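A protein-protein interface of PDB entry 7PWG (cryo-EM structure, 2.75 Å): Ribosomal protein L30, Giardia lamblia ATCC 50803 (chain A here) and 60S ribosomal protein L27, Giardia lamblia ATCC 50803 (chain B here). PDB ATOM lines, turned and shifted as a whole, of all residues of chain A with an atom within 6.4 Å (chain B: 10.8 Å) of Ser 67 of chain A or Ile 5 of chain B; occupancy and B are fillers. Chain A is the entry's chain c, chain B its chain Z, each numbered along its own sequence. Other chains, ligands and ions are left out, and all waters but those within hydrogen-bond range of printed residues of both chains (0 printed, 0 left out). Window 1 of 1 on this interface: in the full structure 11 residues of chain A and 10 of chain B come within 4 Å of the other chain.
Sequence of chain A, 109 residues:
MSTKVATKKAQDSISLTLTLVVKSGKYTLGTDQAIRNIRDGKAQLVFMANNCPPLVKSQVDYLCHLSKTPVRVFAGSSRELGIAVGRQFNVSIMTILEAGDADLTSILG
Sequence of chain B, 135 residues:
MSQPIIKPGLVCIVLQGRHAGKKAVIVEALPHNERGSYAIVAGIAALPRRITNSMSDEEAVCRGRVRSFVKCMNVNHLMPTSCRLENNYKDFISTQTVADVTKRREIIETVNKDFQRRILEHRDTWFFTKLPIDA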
ATOM      1  N   ILE A  38      -0.213   3.431 -34.425  1.00  0.00           N
ATOM      2  CA  ILE A  38      -0.075   3.589 -32.979  1.00  0.00           C
ATOM      3  C   ILE A  38      -0.201   2.247 -32.273  1.00  0.00           C
ATOM      4  O   ILE A  38       0.585   1.927 -31.374  1.00  0.00           O
ATOM      5  CB  ILE A  38      -1.101   4.607 -32.454  1.00  0.00           C
ATOM      6  CG1 ILE A  38      -0.747   6.012 -32.941  1.00  0.00           C
ATOM      7  CG2 ILE A  38      -1.163   4.583 -30.945  1.00  0.00           C
ATOM      8  CD1 ILE A  38      -1.907   6.984 -32.873  1.00  0.00           C
ATOM      9  N   ARG A  39      -1.178   1.432 -32.669  1.00  0.00           N
ATOM     10  CA  ARG A  39      -1.337   0.133 -32.033  1.00  0.00           C
ATOM     11  C   ARG A  39      -0.145  -0.783 -32.279  1.00  0.00           C
ATOM     12  O   ARG A  39       0.038  -1.745 -31.533  1.00  0.00           O
ATOM     13  CB  ARG A  39      -2.632  -0.532 -32.504  1.00  0.00           C
ATOM     14  CG  ARG A  39      -2.522  -1.261 -33.822  1.00  0.00           C
ATOM     15  CD  ARG A  39      -3.886  -1.690 -34.354  1.00  0.00           C
ATOM     16  NE  ARG A  39      -3.754  -2.275 -35.683  1.00  0.00           N
ATOM     17  CZ  ARG A  39      -4.695  -2.242 -36.618  1.00  0.00           C
ATOM     18  NH1 ARG A  39      -5.857  -1.656 -36.382  1.00  0.00           N
ATOM     19  NH2 ARG A  39      -4.464  -2.793 -37.796  1.00  0.00           N
ATOM     20  N   ASP A  40       0.675  -0.494 -33.282  1.00  0.00           N
ATOM     21  CA  ASP A  40       1.858  -1.278 -33.582  1.00  0.00           C
ATOM     22  C   ASP A  40       3.143  -0.630 -33.094  1.00  0.00           C
ATOM     23  O   ASP A  40       4.221  -1.191 -33.305  1.00  0.00           O
ATOM     24  CB  ASP A  40       1.943  -1.529 -35.082  1.00  0.00           C
ATOM     25  CG  ASP A  40       0.739  -2.269 -35.611  1.00  0.00           C
ATOM     26  OD1 ASP A  40       0.143  -3.053 -34.850  1.00  0.00           O
ATOM     27  OD2 ASP A  40       0.393  -2.073 -36.789  1.00  0.00           O
ATOM     28  N   GLY A  41       3.053   0.519 -32.433  1.00  0.00           N
ATOM     29  CA  GLY A  41       4.209   1.163 -31.834  1.00  0.00           C
ATOM     30  C   GLY A  41       5.232   1.719 -32.796  1.00  0.00           C
ATOM     31  O   GLY A  41       6.435   1.649 -32.521  1.00  0.00           O
ATOM     32  N   TYR A  62      -6.842   7.820 -26.030  1.00  0.00           N
ATOM     33  CA  TYR A  62      -6.847   6.572 -25.273  1.00  0.00           C
ATOM     34  C   TYR A  62      -5.838   5.584 -25.839  1.00  0.00           C
ATOM     35  O   TYR A  62      -5.069   4.969 -25.093  1.00  0.00           O
ATOM     36  CB  TYR A  62      -8.241   5.952 -25.249  1.00  0.00           C
ATOM     37  CG  TYR A  62      -8.404   4.991 -24.100  1.00  0.00           C
ATOM     38  CD1 TYR A  62      -8.063   3.655 -24.228  1.00  0.00           C
ATOM     39  CD2 TYR A  62      -8.849   5.435 -22.864  1.00  0.00           C
ATOM     40  CE1 TYR A  62      -8.192   2.789 -23.166  1.00  0.00           C
ATOM     41  CE2 TYR A  62      -8.978   4.579 -21.801  1.00  0.00           C
ATOM     42  CZ  TYR A  62      -8.654   3.262 -21.954  1.00  0.00           C
ATOM     43  OH  TYR A  62      -8.795   2.418 -20.883  1.00  0.00           O
ATOM     44  N   LEU A  63      -5.817   5.432 -27.163  1.00  0.00           N
ATOM     45  CA  LEU A  63      -4.832   4.563 -27.790  1.00  0.00           C
ATOM     46  C   LEU A  63      -3.413   5.058 -27.570  1.00  0.00           C
ATOM     47  O   LEU A  63      -2.472   4.263 -27.612  1.00  0.00           O
ATOM     48  CB  LEU A  63      -5.100   4.451 -29.287  1.00  0.00           C
ATOM     49  CG  LEU A  63      -6.273   3.608 -29.755  1.00  0.00           C
ATOM     50  CD1 LEU A  63      -6.272   3.581 -31.259  1.00  0.00           C
ATOM     51  CD2 LEU A  63      -6.163   2.212 -29.193  1.00  0.00           C
ATOM     52  N   CYS A  64      -3.232   6.365 -27.380  1.00  0.00           N
ATOM     53  CA  CYS A  64      -1.889   6.905 -27.214  1.00  0.00           C
ATOM     54  C   CYS A  64      -1.329   6.591 -25.836  1.00  0.00           C
ATOM     55  O   CYS A  64      -0.167   6.198 -25.713  1.00  0.00           O
ATOM     56  CB  CYS A  64      -1.885   8.411 -27.464  1.00  0.00           C
ATOM     57  SG  CYS A  64      -1.662   8.869 -29.190  1.00  0.00           S
ATOM     58  N   HIS A  65      -2.143   6.747 -24.794  1.00  0.00           N
ATOM     59  CA  HIS A  65      -1.681   6.494 -23.434  1.00  0.00           C
ATOM     60  C   HIS A  65      -1.337   5.028 -23.217  1.00  0.00           C
ATOM     61  O   HIS A  65      -0.444   4.717 -22.423  1.00  0.00           O
ATOM     62  CB  HIS A  65      -2.741   6.964 -22.439  1.00  0.00           C
ATOM     63  CG  HIS A  65      -2.699   6.260 -21.119  1.00  0.00           C
ATOM     64  ND1 HIS A  65      -3.338   5.061 -20.894  1.00  0.00           N
ATOM     65  CD2 HIS A  65      -2.109   6.594 -19.948  1.00  0.00           C
ATOM     66  CE1 HIS A  65      -3.140   4.684 -19.645  1.00  0.00           C
ATOM     67  NE2 HIS A  65      -2.394   5.596 -19.050  1.00  0.00           N
ATOM     68  N   LEU A  66      -2.027   4.116 -23.903  1.00  0.00           N
ATOM     69  CA  LEU A  66      -1.671   2.708 -23.796  1.00  0.00           C
ATOM     70  C   LEU A  66      -0.334   2.414 -24.455  1.00  0.00           C
ATOM     71  O   LEU A  66       0.399   1.534 -23.994  1.00  0.00           O
ATOM     72  CB  LEU A  66      -2.749   1.825 -24.418  1.00  0.00           C
ATOM     73  CG  LEU A  66      -4.141   1.742 -23.807  1.00  0.00           C
ATOM     74  CD1 LEU A  66      -4.959   0.736 -24.585  1.00  0.00           C
ATOM     75  CD2 LEU A  66      -4.094   1.370 -22.340  1.00  0.00           C
ATOM     76  N   SER A  67      -0.011   3.106 -25.543  1.00  0.00           N
ATOM     77  CA  SER A  67       1.242   2.867 -26.236  1.00  0.00           C
ATOM     78  C   SER A  67       2.361   3.789 -25.785  1.00  0.00           C
ATOM     79  O   SER A  67       3.510   3.570 -26.180  1.00  0.00           O
ATOM     80  CB  SER A  67       1.051   3.013 -27.747  1.00  0.00           C
ATOM     81  OG  SER A  67       0.655   4.330 -28.082  1.00  0.00           O
ATOM     82  N   LYS A  68       2.058   4.792 -24.961  1.00  0.00           N
ATOM     83  CA  LYS A  68       3.001   5.828 -24.545  1.00  0.00           C
ATOM     84  C   LYS A  68       3.449   6.706 -25.706  1.00  0.00           C
ATOM     85  O   LYS A  68       4.511   7.331 -25.635  1.00  0.00           O
ATOM     86  CB  LYS A  68       4.229   5.236 -23.835  1.00  0.00           C
ATOM     87  CG  LYS A  68       3.905   4.266 -22.720  1.00  0.00           C
ATOM     88  CD  LYS A  68       2.806   4.793 -21.803  1.00  0.00           C
ATOM     89  CE  LYS A  68       2.529   3.840 -20.651  1.00  0.00           C
ATOM     90  NZ  LYS A  68       2.339   2.434 -21.093  1.00  0.00           N
ATOM     91  N   THR A  69       2.658   6.758 -26.771  1.00  0.00           N
ATOM     92  CA  THR A  69       2.922   7.634 -27.907  1.00  0.00           C
ATOM     93  C   THR A  69       2.510   9.060 -27.564  1.00  0.00           C
ATOM     94  O   THR A  69       1.332   9.298 -27.284  1.00  0.00           O
ATOM     95  CB  THR A  69       2.142   7.162 -29.135  1.00  0.00           C
ATOM     96  OG1 THR A  69       0.827   6.757 -28.738  1.00  0.00           O
ATOM     97  CG2 THR A  69       2.812   5.987 -29.809  1.00  0.00           C
ATOM     98  N   PRO A  70       3.427  10.027 -27.585  1.00  0.00           N
ATOM     99  CA  PRO A  70       3.043  11.423 -27.328  1.00  0.00           C
ATOM    100  C   PRO A  70       2.031  11.938 -28.344  1.00  0.00           C
ATOM    101  O   PRO A  70       2.097  11.615 -29.530  1.00  0.00           O
ATOM    102  CB  PRO A  70       4.370  12.181 -27.446  1.00  0.00           C
ATOM    103  CG  PRO A  70       5.439  11.151 -27.357  1.00  0.00           C
ATOM    104  CD  PRO A  70       4.871   9.873 -27.832  1.00  0.00           C
ATOM    105  N   SER B   2       5.318   4.272 -28.921  1.00  0.00           N
ATOM    106  CA  SER B   2       6.501   3.725 -28.286  1.00  0.00           C
ATOM    107  C   SER B   2       6.529   2.200 -28.342  1.00  0.00           C
ATOM    108  O   SER B   2       7.512   1.626 -28.809  1.00  0.00           O
ATOM    109  CB  SER B   2       6.599   4.197 -26.842  1.00  0.00           C
ATOM    110  OG  SER B   2       6.949   5.560 -26.772  1.00  0.00           O
ATOM    111  N   GLN B   3       5.459   1.546 -27.878  1.00  0.00           N
ATOM    112  CA  GLN B   3       5.457   0.092 -27.759  1.00  0.00           C
ATOM    113  C   GLN B   3       4.190  -0.535 -28.326  1.00  0.00           C
ATOM    114  O   GLN B   3       3.096   0.014 -28.167  1.00  0.00           O
ATOM    115  CB  GLN B   3       5.593  -0.333 -26.296  1.00  0.00           C
ATOM    116  CG  GLN B   3       6.802   0.212 -25.601  1.00  0.00           C
ATOM    117  CD  GLN B   3       7.114  -0.554 -24.348  1.00  0.00           C
ATOM    118  OE1 GLN B   3       6.505  -0.330 -23.302  1.00  0.00           O
ATOM    119  NE2 GLN B   3       8.062  -1.479 -24.445  1.00  0.00           N
ATOM    120  N   PRO B   4       4.305  -1.701 -28.957  1.00  0.00           N
ATOM    121  CA  PRO B   4       3.110  -2.407 -29.435  1.00  0.00           C
ATOM    122  C   PRO B   4       2.226  -2.842 -28.280  1.00  0.00           C
ATOM    123  O   PRO B   4       2.699  -3.094 -27.170  1.00  0.00           O
ATOM    124  CB  PRO B   4       3.686  -3.616 -30.175  1.00  0.00           C
ATOM    125  CG  PRO B   4       5.061  -3.779 -29.610  1.00  0.00           C
ATOM    126  CD  PRO B   4       5.543  -2.413 -29.307  1.00  0.00           C
ATOM    127  N   ILE B   5       0.928  -2.920 -28.551  1.00  0.00           N
ATOM    128  CA  ILE B   5      -0.050  -3.230 -27.519  1.00  0.00           C
ATOM    129  C   ILE B   5      -0.888  -4.461 -27.833  1.00  0.00           C
ATOM    130  O   ILE B   5      -1.461  -5.051 -26.904  1.00  0.00           O
ATOM    131  CB  ILE B   5      -0.971  -2.025 -27.245  1.00  0.00           C
ATOM    132  CG1 ILE B   5      -2.178  -2.055 -28.178  1.00  0.00           C
ATOM    133  CG2 ILE B   5      -0.214  -0.722 -27.414  1.00  0.00           C
ATOM    134  CD1 ILE B   5      -2.885  -0.745 -28.286  1.00  0.00           C
ATOM    135  N   ILE B   6      -0.987  -4.898 -29.085  1.00  0.00           N
ATOM    136  CA  ILE B   6      -1.785  -6.080 -29.381  1.00  0.00           C
ATOM    137  C   ILE B   6      -0.959  -7.288 -28.972  1.00  0.00           C
ATOM    138  O   ILE B   6      -0.204  -7.846 -29.773  1.00  0.00           O
ATOM    139  CB  ILE B   6      -2.186  -6.155 -30.864  1.00  0.00           C
ATOM    140  CG1 ILE B   6      -2.726  -4.813 -31.352  1.00  0.00           C
ATOM    141  CG2 ILE B   6      -3.217  -7.260 -31.095  1.00  0.00           C
ATOM    142  CD1 ILE B   6      -4.046  -4.417 -30.743  1.00  0.00           C
ATOM    143  N   LYS B   7      -1.102  -7.694 -27.721  1.00  0.00           N
ATOM    144  CA  LYS B   7      -0.359  -8.787 -27.126  1.00  0.00           C
ATOM    145  C   LYS B   7      -1.344  -9.791 -26.555  1.00  0.00           C
ATOM    146  O   LYS B   7      -2.453  -9.415 -26.165  1.00  0.00           O
ATOM    147  CB  LYS B   7       0.563  -8.289 -26.003  1.00  0.00           C
ATOM    148  CG  LYS B   7       1.686  -7.391 -26.460  1.00  0.00           C
ATOM    149  CD  LYS B   7       1.540  -6.008 -25.872  1.00  0.00           C
ATOM    150  CE  LYS B   7       1.393  -6.039 -24.357  1.00  0.00           C
ATOM    151  NZ  LYS B   7       0.803  -4.772 -23.835  1.00  0.00           N
ATOM    152  N   PRO B   8      -0.967 -11.065 -26.490  1.00  0.00           N
ATOM    153  CA  PRO B   8      -1.858 -12.060 -25.889  1.00  0.00           C
ATOM    154  C   PRO B   8      -2.166 -11.718 -24.443  1.00  0.00           C
ATOM    155  O   PRO B   8      -1.297 -11.278 -23.691  1.00  0.00           O
ATOM    156  CB  PRO B   8      -1.067 -13.366 -26.007  1.00  0.00           C
ATOM    157  CG  PRO B   8       0.320 -12.961 -26.250  1.00  0.00           C
ATOM    158  CD  PRO B   8       0.258 -11.680 -27.010  1.00  0.00           C
ATOM    159  N   GLY B   9      -3.421 -11.918 -24.066  1.00  0.00           N
ATOM    160  CA  GLY B   9      -3.904 -11.583 -22.752  1.00  0.00           C
ATOM    161  C   GLY B   9      -4.703 -10.305 -22.674  1.00  0.00           C
ATOM    162  O   GLY B   9      -5.366 -10.079 -21.661  1.00  0.00           O
ATOM    163  N   LEU B  10      -4.670  -9.478 -23.710  1.00  0.00           N
ATOM    164  CA  LEU B  10      -5.389  -8.212 -23.718  1.00  0.00           C
ATOM    165  C   LEU B  10      -6.881  -8.435 -23.954  1.00  0.00           C
ATOM    166  O   LEU B  10      -7.291  -9.392 -24.612  1.00  0.00           O
ATOM    167  CB  LEU B  10      -4.801  -7.297 -24.792  1.00  0.00           C
ATOM    168  CG  LEU B  10      -5.448  -5.970 -25.185  1.00  0.00           C
ATOM    169  CD1 LEU B  10      -5.373  -4.956 -24.074  1.00  0.00           C
ATOM    170  CD2 LEU B  10      -4.797  -5.433 -26.444  1.00  0.00           C
ATOM    171  N   VAL B  11      -7.694  -7.552 -23.385  1.00  0.00           N
ATOM    172  CA  VAL B  11      -9.145  -7.597 -23.530  1.00  0.00           C
ATOM    173  C   VAL B  11      -9.570  -6.504 -24.501  1.00  0.00           C
ATOM    174  O   VAL B  11      -9.175  -5.342 -24.352  1.00  0.00           O
ATOM    175  CB  VAL B  11      -9.851  -7.432 -22.172  1.00  0.00           C
ATOM    176  CG1 VAL B  11     -11.335  -7.227 -22.368  1.00  0.00           C
ATOM    177  CG2 VAL B  11      -9.609  -8.634 -21.299  1.00  0.00           C
ATOM    178  N   CYS B  12     -10.366  -6.873 -25.497  1.00  0.00           N
ATOM    179  CA  CYS B  12     -10.871  -5.941 -26.490  1.00  0.00           C
ATOM    180  C   CYS B  12     -12.392  -5.917 -26.462  1.00  0.00           C
ATOM    181  O   CYS B  12     -13.037  -6.829 -25.946  1.00  0.00           O
ATOM    182  CB  CYS B  12     -10.386  -6.310 -27.893  1.00  0.00           C
ATOM    183  SG  CYS B  12      -8.657  -5.971 -28.198  1.00  0.00           S
ATOM    184  N   VAL B  25     -11.038 -11.858 -25.430  1.00  0.00           N
ATOM    185  CA  VAL B  25      -9.609 -11.898 -25.142  1.00  0.00           C
ATOM    186  C   VAL B  25      -8.871 -12.199 -26.441  1.00  0.00           C
ATOM    187  O   VAL B  25      -9.428 -12.756 -27.385  1.00  0.00           O
ATOM    188  CB  VAL B  25      -9.273 -12.958 -24.070  1.00  0.00           C
ATOM    189  CG1 VAL B  25      -8.013 -12.609 -23.333  1.00  0.00           C
ATOM    190  CG2 VAL B  25     -10.428 -13.115 -23.107  1.00  0.00           C
ATOM    191  N   ILE B  26      -7.600 -11.831 -26.485  1.00  0.00           N
ATOM    192  CA  ILE B  26      -6.751 -12.150 -27.625  1.00  0.00           C
ATOM    193  C   ILE B  26      -5.953 -13.392 -27.267  1.00  0.00           C
ATOM    194  O   ILE B  26      -5.044 -13.344 -26.435  1.00  0.00           O
ATOM    195  CB  ILE B  26      -5.842 -10.977 -28.013  1.00  0.00           C
ATOM    196  CG1 ILE B  26      -6.674  -9.867 -28.657  1.00  0.00           C
ATOM    197  CG2 ILE B  26      -4.782 -11.425 -28.988  1.00  0.00           C
ATOM    198  CD1 ILE B  26      -5.924  -8.571 -28.831  1.00  0.00           C
ATOM    199  N   VAL B  27      -6.322 -14.512 -27.886  1.00  0.00           N
ATOM    200  CA  VAL B  27      -5.569 -15.752 -27.742  1.00  0.00           C
ATOM    201  C   VAL B  27      -4.210 -15.638 -28.423  1.00  0.00           C
ATOM    202  O   VAL B  27      -3.202 -16.140 -27.913  1.00  0.00           O
ATOM    203  CB  VAL B  27      -6.391 -16.928 -28.304  1.00  0.00           C
ATOM    204  CG1 VAL B  27      -5.591 -18.223 -28.300  1.00  0.00           C
ATOM    205  CG2 VAL B  27      -7.686 -17.103 -27.522  1.00  0.00           C
ATOM    206  N   GLU B  28      -4.155 -14.983 -29.581  1.00  0.00           N
ATOM    207  CA  GLU B  28      -2.958 -15.013 -30.411  1.00  0.00           C
ATOM    208  C   GLU B  28      -2.970 -13.846 -31.388  1.00  0.00           C
ATOM    209  O   GLU B  28      -4.013 -13.515 -31.950  1.00  0.00           O
ATOM    210  CB  GLU B  28      -2.880 -16.329 -31.181  1.00  0.00           C
ATOM    211  CG  GLU B  28      -1.524 -16.623 -31.729  1.00  0.00           C
ATOM    212  CD  GLU B  28      -1.510 -17.880 -32.544  1.00  0.00           C
ATOM    213  OE1 GLU B  28      -0.945 -17.851 -33.653  1.00  0.00           O
ATOM    214  OE2 GLU B  28      -2.070 -18.899 -32.076  1.00  0.00           O
ATOM    215  N   ALA B  29      -1.805 -13.245 -31.607  1.00  0.00           N
ATOM    216  CA  ALA B  29      -1.670 -12.087 -32.492  1.00  0.00           C
ATOM    217  C   ALA B  29      -1.002 -12.528 -33.790  1.00  0.00           C
ATOM    218  O   ALA B  29       0.225 -12.530 -33.898  1.00  0.00           O
ATOM    219  CB  ALA B  29      -0.879 -10.981 -31.804  1.00  0.00           C
ATOM    220  N   ALA B  39      -6.393 -11.794 -35.478  1.00  0.00           N
ATOM    221  CA  ALA B  39      -6.074 -12.352 -34.172  1.00  0.00           C
ATOM    222  C   ALA B  39      -7.101 -13.415 -33.822  1.00  0.00           C
ATOM    223  O   ALA B  39      -8.283 -13.259 -34.119  1.00  0.00           O
ATOM    224  CB  ALA B  39      -6.051 -11.265 -33.089  1.00  0.00           C
ATOM    225  N   VAL B  75      -8.312  -6.857 -36.760  1.00  0.00           N
ATOM    226  CA  VAL B  75      -7.956  -5.966 -35.664  1.00  0.00           C
ATOM    227  C   VAL B  75      -8.511  -4.560 -35.849  1.00  0.00           C
ATOM    228  O   VAL B  75      -8.638  -3.819 -34.871  1.00  0.00           O
ATOM    229  CB  VAL B  75      -6.428  -5.931 -35.491  1.00  0.00           C
ATOM    230  CG1 VAL B  75      -6.051  -5.191 -34.228  1.00  0.00           C
ATOM    231  CG2 VAL B  75      -5.883  -7.332 -35.456  1.00  0.00           C
ATOM    232  N   LEU B  78     -11.560  -4.133 -33.563  1.00  0.00           N
ATOM    233  CA  LEU B  78     -11.357  -4.297 -32.127  1.00  0.00           C
ATOM    234  C   LEU B  78     -10.958  -2.974 -31.489  1.00  0.00           C
ATOM    235  O   LEU B  78     -10.210  -2.192 -32.078  1.00  0.00           O
ATOM    236  CB  LEU B  78     -10.274  -5.344 -31.835  1.00  0.00           C
ATOM    237  CG  LEU B  78     -10.669  -6.785 -31.516  1.00  0.00           C
ATOM    238  CD1 LEU B  78     -11.848  -7.254 -32.317  1.00  0.00           C
ATOM    239  CD2 LEU B  78      -9.495  -7.689 -31.775  1.00  0.00           C
ATOM    240  N   MET B  79     -11.469  -2.728 -30.289  1.00  0.00           N
ATOM    241  CA  MET B  79     -11.021  -1.626 -29.441  1.00  0.00           C
ATOM    242  C   MET B  79     -10.410  -2.198 -28.175  1.00  0.00           C
ATOM    243  O   MET B  79     -11.138  -2.783 -27.353  1.00  0.00           O
ATOM    244  CB  MET B  79     -12.175  -0.688 -29.092  1.00  0.00           C
ATOM    245  CG  MET B  79     -11.780   0.513 -28.236  1.00  0.00           C
ATOM    246  SD  MET B  79     -10.520   1.540 -29.007  1.00  0.00           S
ATOM    247  CE  MET B  79     -10.424   2.886 -27.828  1.00  0.00           C
ATOM    248  N   PRO B  80      -9.107  -2.083 -27.965  1.00  0.00           N
ATOM    249  CA  PRO B  80      -8.495  -2.631 -26.753  1.00  0.00           C
ATOM    250  C   PRO B  80      -8.782  -1.774 -25.525  1.00  0.00           C
ATOM    251  O   PRO B  80      -9.327  -0.674 -25.604  1.00  0.00           O
ATOM    252  CB  PRO B  80      -7.007  -2.637 -27.093  1.00  0.00           C
ATOM    253  CG  PRO B  80      -6.850  -1.613 -28.130  1.00  0.00           C
ATOM    254  CD  PRO B  80      -8.094  -1.636 -28.935  1.00  0.00           C
ATOM    255  N   THR B  81      -8.400  -2.315 -24.369  1.00  0.00           N
ATOM    256  CA  THR B  81      -8.642  -1.703 -23.071  1.00  0.00           C
ATOM    257  C   THR B  81      -7.373  -1.750 -22.232  1.00  0.00           C
ATOM    258  O   THR B  81      -6.327  -2.239 -22.664  1.00  0.00           O
ATOM    259  CB  THR B  81      -9.765  -2.413 -22.303  1.00  0.00           C
ATOM    260  OG1 THR B  81      -9.337  -3.738 -21.978  1.00  0.00           O
ATOM    261  CG2 THR B  81     -11.038  -2.482 -23.111  1.00  0.00           C
ATOM    262  N   SER B  82      -7.481  -1.243 -21.005  1.00  0.00           N
ATOM    263  CA  SER B  82      -6.451  -1.483 -20.000  1.00  0.00           C
ATOM    264  C   SER B  82      -6.543  -2.892 -19.425  1.00  0.00           C
ATOM    265  O   SER B  82      -5.513  -3.499 -19.111  1.00  0.00           O
ATOM    266  CB  SER B  82      -6.568  -0.460 -18.870  1.00  0.00           C
ATOM    267  OG  SER B  82      -6.565   0.865 -19.359  1.00  0.00           O
ATOM    268  N   CYS B  83      -7.752  -3.435 -19.325  1.00  0.00           N
ATOM    269  CA  CYS B  83      -7.999  -4.666 -18.588  1.00  0.00           C
ATOM    270  C   CYS B  83      -7.242  -5.847 -19.193  1.00  0.00           C
ATOM    271  O   CYS B  83      -6.811  -5.832 -20.347  1.00  0.00           O
ATOM    272  CB  CYS B  83      -9.497  -4.956 -18.543  1.00  0.00           C
ATOM    273  SG  CYS B  83      -9.948  -6.511 -17.740  1.00  0.00           S
ATOM    274  N   ARG B  84      -7.082  -6.882 -18.376  1.00  0.00           N
ATOM    275  CA  ARG B  84      -6.150  -7.970 -18.617  1.00  0.00           C
ATOM    276  C   ARG B  84      -6.827  -9.265 -18.194  1.00  0.00           C
ATOM    277  O   ARG B  84      -7.754  -9.256 -17.385  1.00  0.00           O
ATOM    278  CB  ARG B  84      -4.850  -7.740 -17.822  1.00  0.00           C
ATOM    279  CG  ARG B  84      -3.656  -8.565 -18.239  1.00  0.00           C
ATOM    280  CD  ARG B  84      -2.962  -7.952 -19.423  1.00  0.00           C
ATOM    281  NE  ARG B  84      -2.559  -8.987 -20.358  1.00  0.00           N
ATOM    282  CZ  ARG B  84      -1.334  -9.481 -20.438  1.00  0.00           C
ATOM    283  NH1 ARG B  84      -0.382  -9.009 -19.649  1.00  0.00           N
ATOM    284  NH2 ARG B  84      -1.065 -10.434 -21.314  1.00  0.00           N
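Arg 39 of chain A touches Pro 4 of chain B.
Arg 39 of chain A touches Val 75 of chain B.
Asp 40 of chain A touches Pro 4 of chain B (O to CB, 3.995 Å).
O of Gly 41 of chain A touches O of Ser 2 of chain B, at 3.9 Å.
Gly 41 of chain A touches Gln 3 of chain B.
CD1 of Leu 66 of chain A touches O of Thr 81 of chain B, at 3.8 Å.
OG of Ser 82 of chain B touches CD2 of Leu 66 of chain A, 3.9 Å away.
CB of Ser 67 of chain A touches CG2 of Ile 5 of chain B, at 3.96 Å.
Thr 69 of chain A touches Ser 2 of chain B (CG2 to N, 3.2 Å).
Ser 67 of chain A touches just these residues of chain B: Ser 2 (3.2 Å), Gln 3 (3.3 Å) and Ile 5 (3.96 Å).
Ile 5 of chain B touches just these residues of chain A: Arg 39 (3.3 Å) and Ser 67 (3.96 Å).
Ile 38 of chain A touches none of the printed residues of chain B.
No residue of chain B comes within 4 Å of Leu 63 of chain A.
No residue of chain B comes within 4 Å of Cys 64 of chain A.
Of chain B, only Thr 81 and Ser 82 come within 4 Å of Leu 66 of chain A.
Printed residues of chain B within 4 Å of Lys 68 of chain A: Ser 2.
Of the printed residues of chain B, Thr 69 of chain A touches Ser 2 (3.2 Å).
Printed residues of chain A within 4 Å of Thr 81 of chain B: Leu 66.
Printed residues of chain A within 4 Å of Gln 3 of chain B: Gly 41 and Ser 67.
Of the printed residues of chain A, Val 75 of chain B touches Arg 39.
Arg 84 of chain B touches none of the printed residues of chain A.
The nearest residue of chain B that does not touch Ser 67 of chain A is Pro 4 of chain B (5.9 Å).
The nearest residue of chain A that does not touch Ile 5 of chain B is Leu 66 of chain A (4.1 Å).
Printed residues of chain B that touch a printed residue of chain A: Ser 2, Gln 3, Pro 4, Ile 5, Val 75, Thr 81 and Ser 82.
Hydrophobic or aromatic side chains of chain B that line the printed part of chain A: Pro 4, Ile 5 and Val 75.
Of the 13 printed residues of chain A, 8 touch a printed residue of chain B.
Hydrophobic or aromatic side chains of chain A that line the printed part of chain B: Tyr 62 and Leu 66.
Among the printed residues, no Asp or Glu carboxylate lies within 4 Å of a Lys or Arg side-chain nitrogen of the other chain.
The backbone carbonyl oxygen (O) of Ser 67 of chain A lies close to the backbone NH (N) of Ser 2 of chain B.
OG of Ser 2 of chain B sits at hydrogen-bond distance from O of Lys 68 of chain A (3.2 Å).
N of Gln 3 of chain B sits at hydrogen-bond distance from O of Ser 67 of chain A (3.3 Å).
The backbone carbonyl oxygen (O) of Arg 39 of chain A is in hydrogen-bond range of the backbone NH (N) of Ile 5 of chain B (3.3 Å).
The side-chain hydroxyl (OH) of Tyr 62 of chain A sits at hydrogen-bond distance from the side-chain hydroxyl (OG) of Ser 82 of chain B (3.1 Å).
OG1 of Thr 81 of chain B is in hydrogen-bond range of O of Val 11 of chain B (2.9 Å).
OG1 of Thr 81 of chain B lies within hydrogen-bond range of N of Cys 83 of chain B, at 3.1 Å.
The backbone carbonyl oxygen (O) of Leu 63 of chain A lies within hydrogen-bond range of the side-chain hydroxyl (OG) of Ser 67 of chain A, 3.2 Å away.
The side-chain hydroxyl (OG) of Ser 67 of chain A is in hydrogen-bond range of the backbone carbonyl oxygen (O) of Cys 64 of chain A.
The backbone NH (N) of Thr 69 of chain A lies within hydrogen-bond range of the backbone carbonyl oxygen (O) of Cys 64 of chain A (3.1 Å).
The side-chain hydroxyl (OG1) of Thr 69 of chain A lies within hydrogen-bond range of the side-chain hydroxyl (OG) of Ser 67 of chain A (2.5 Å).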
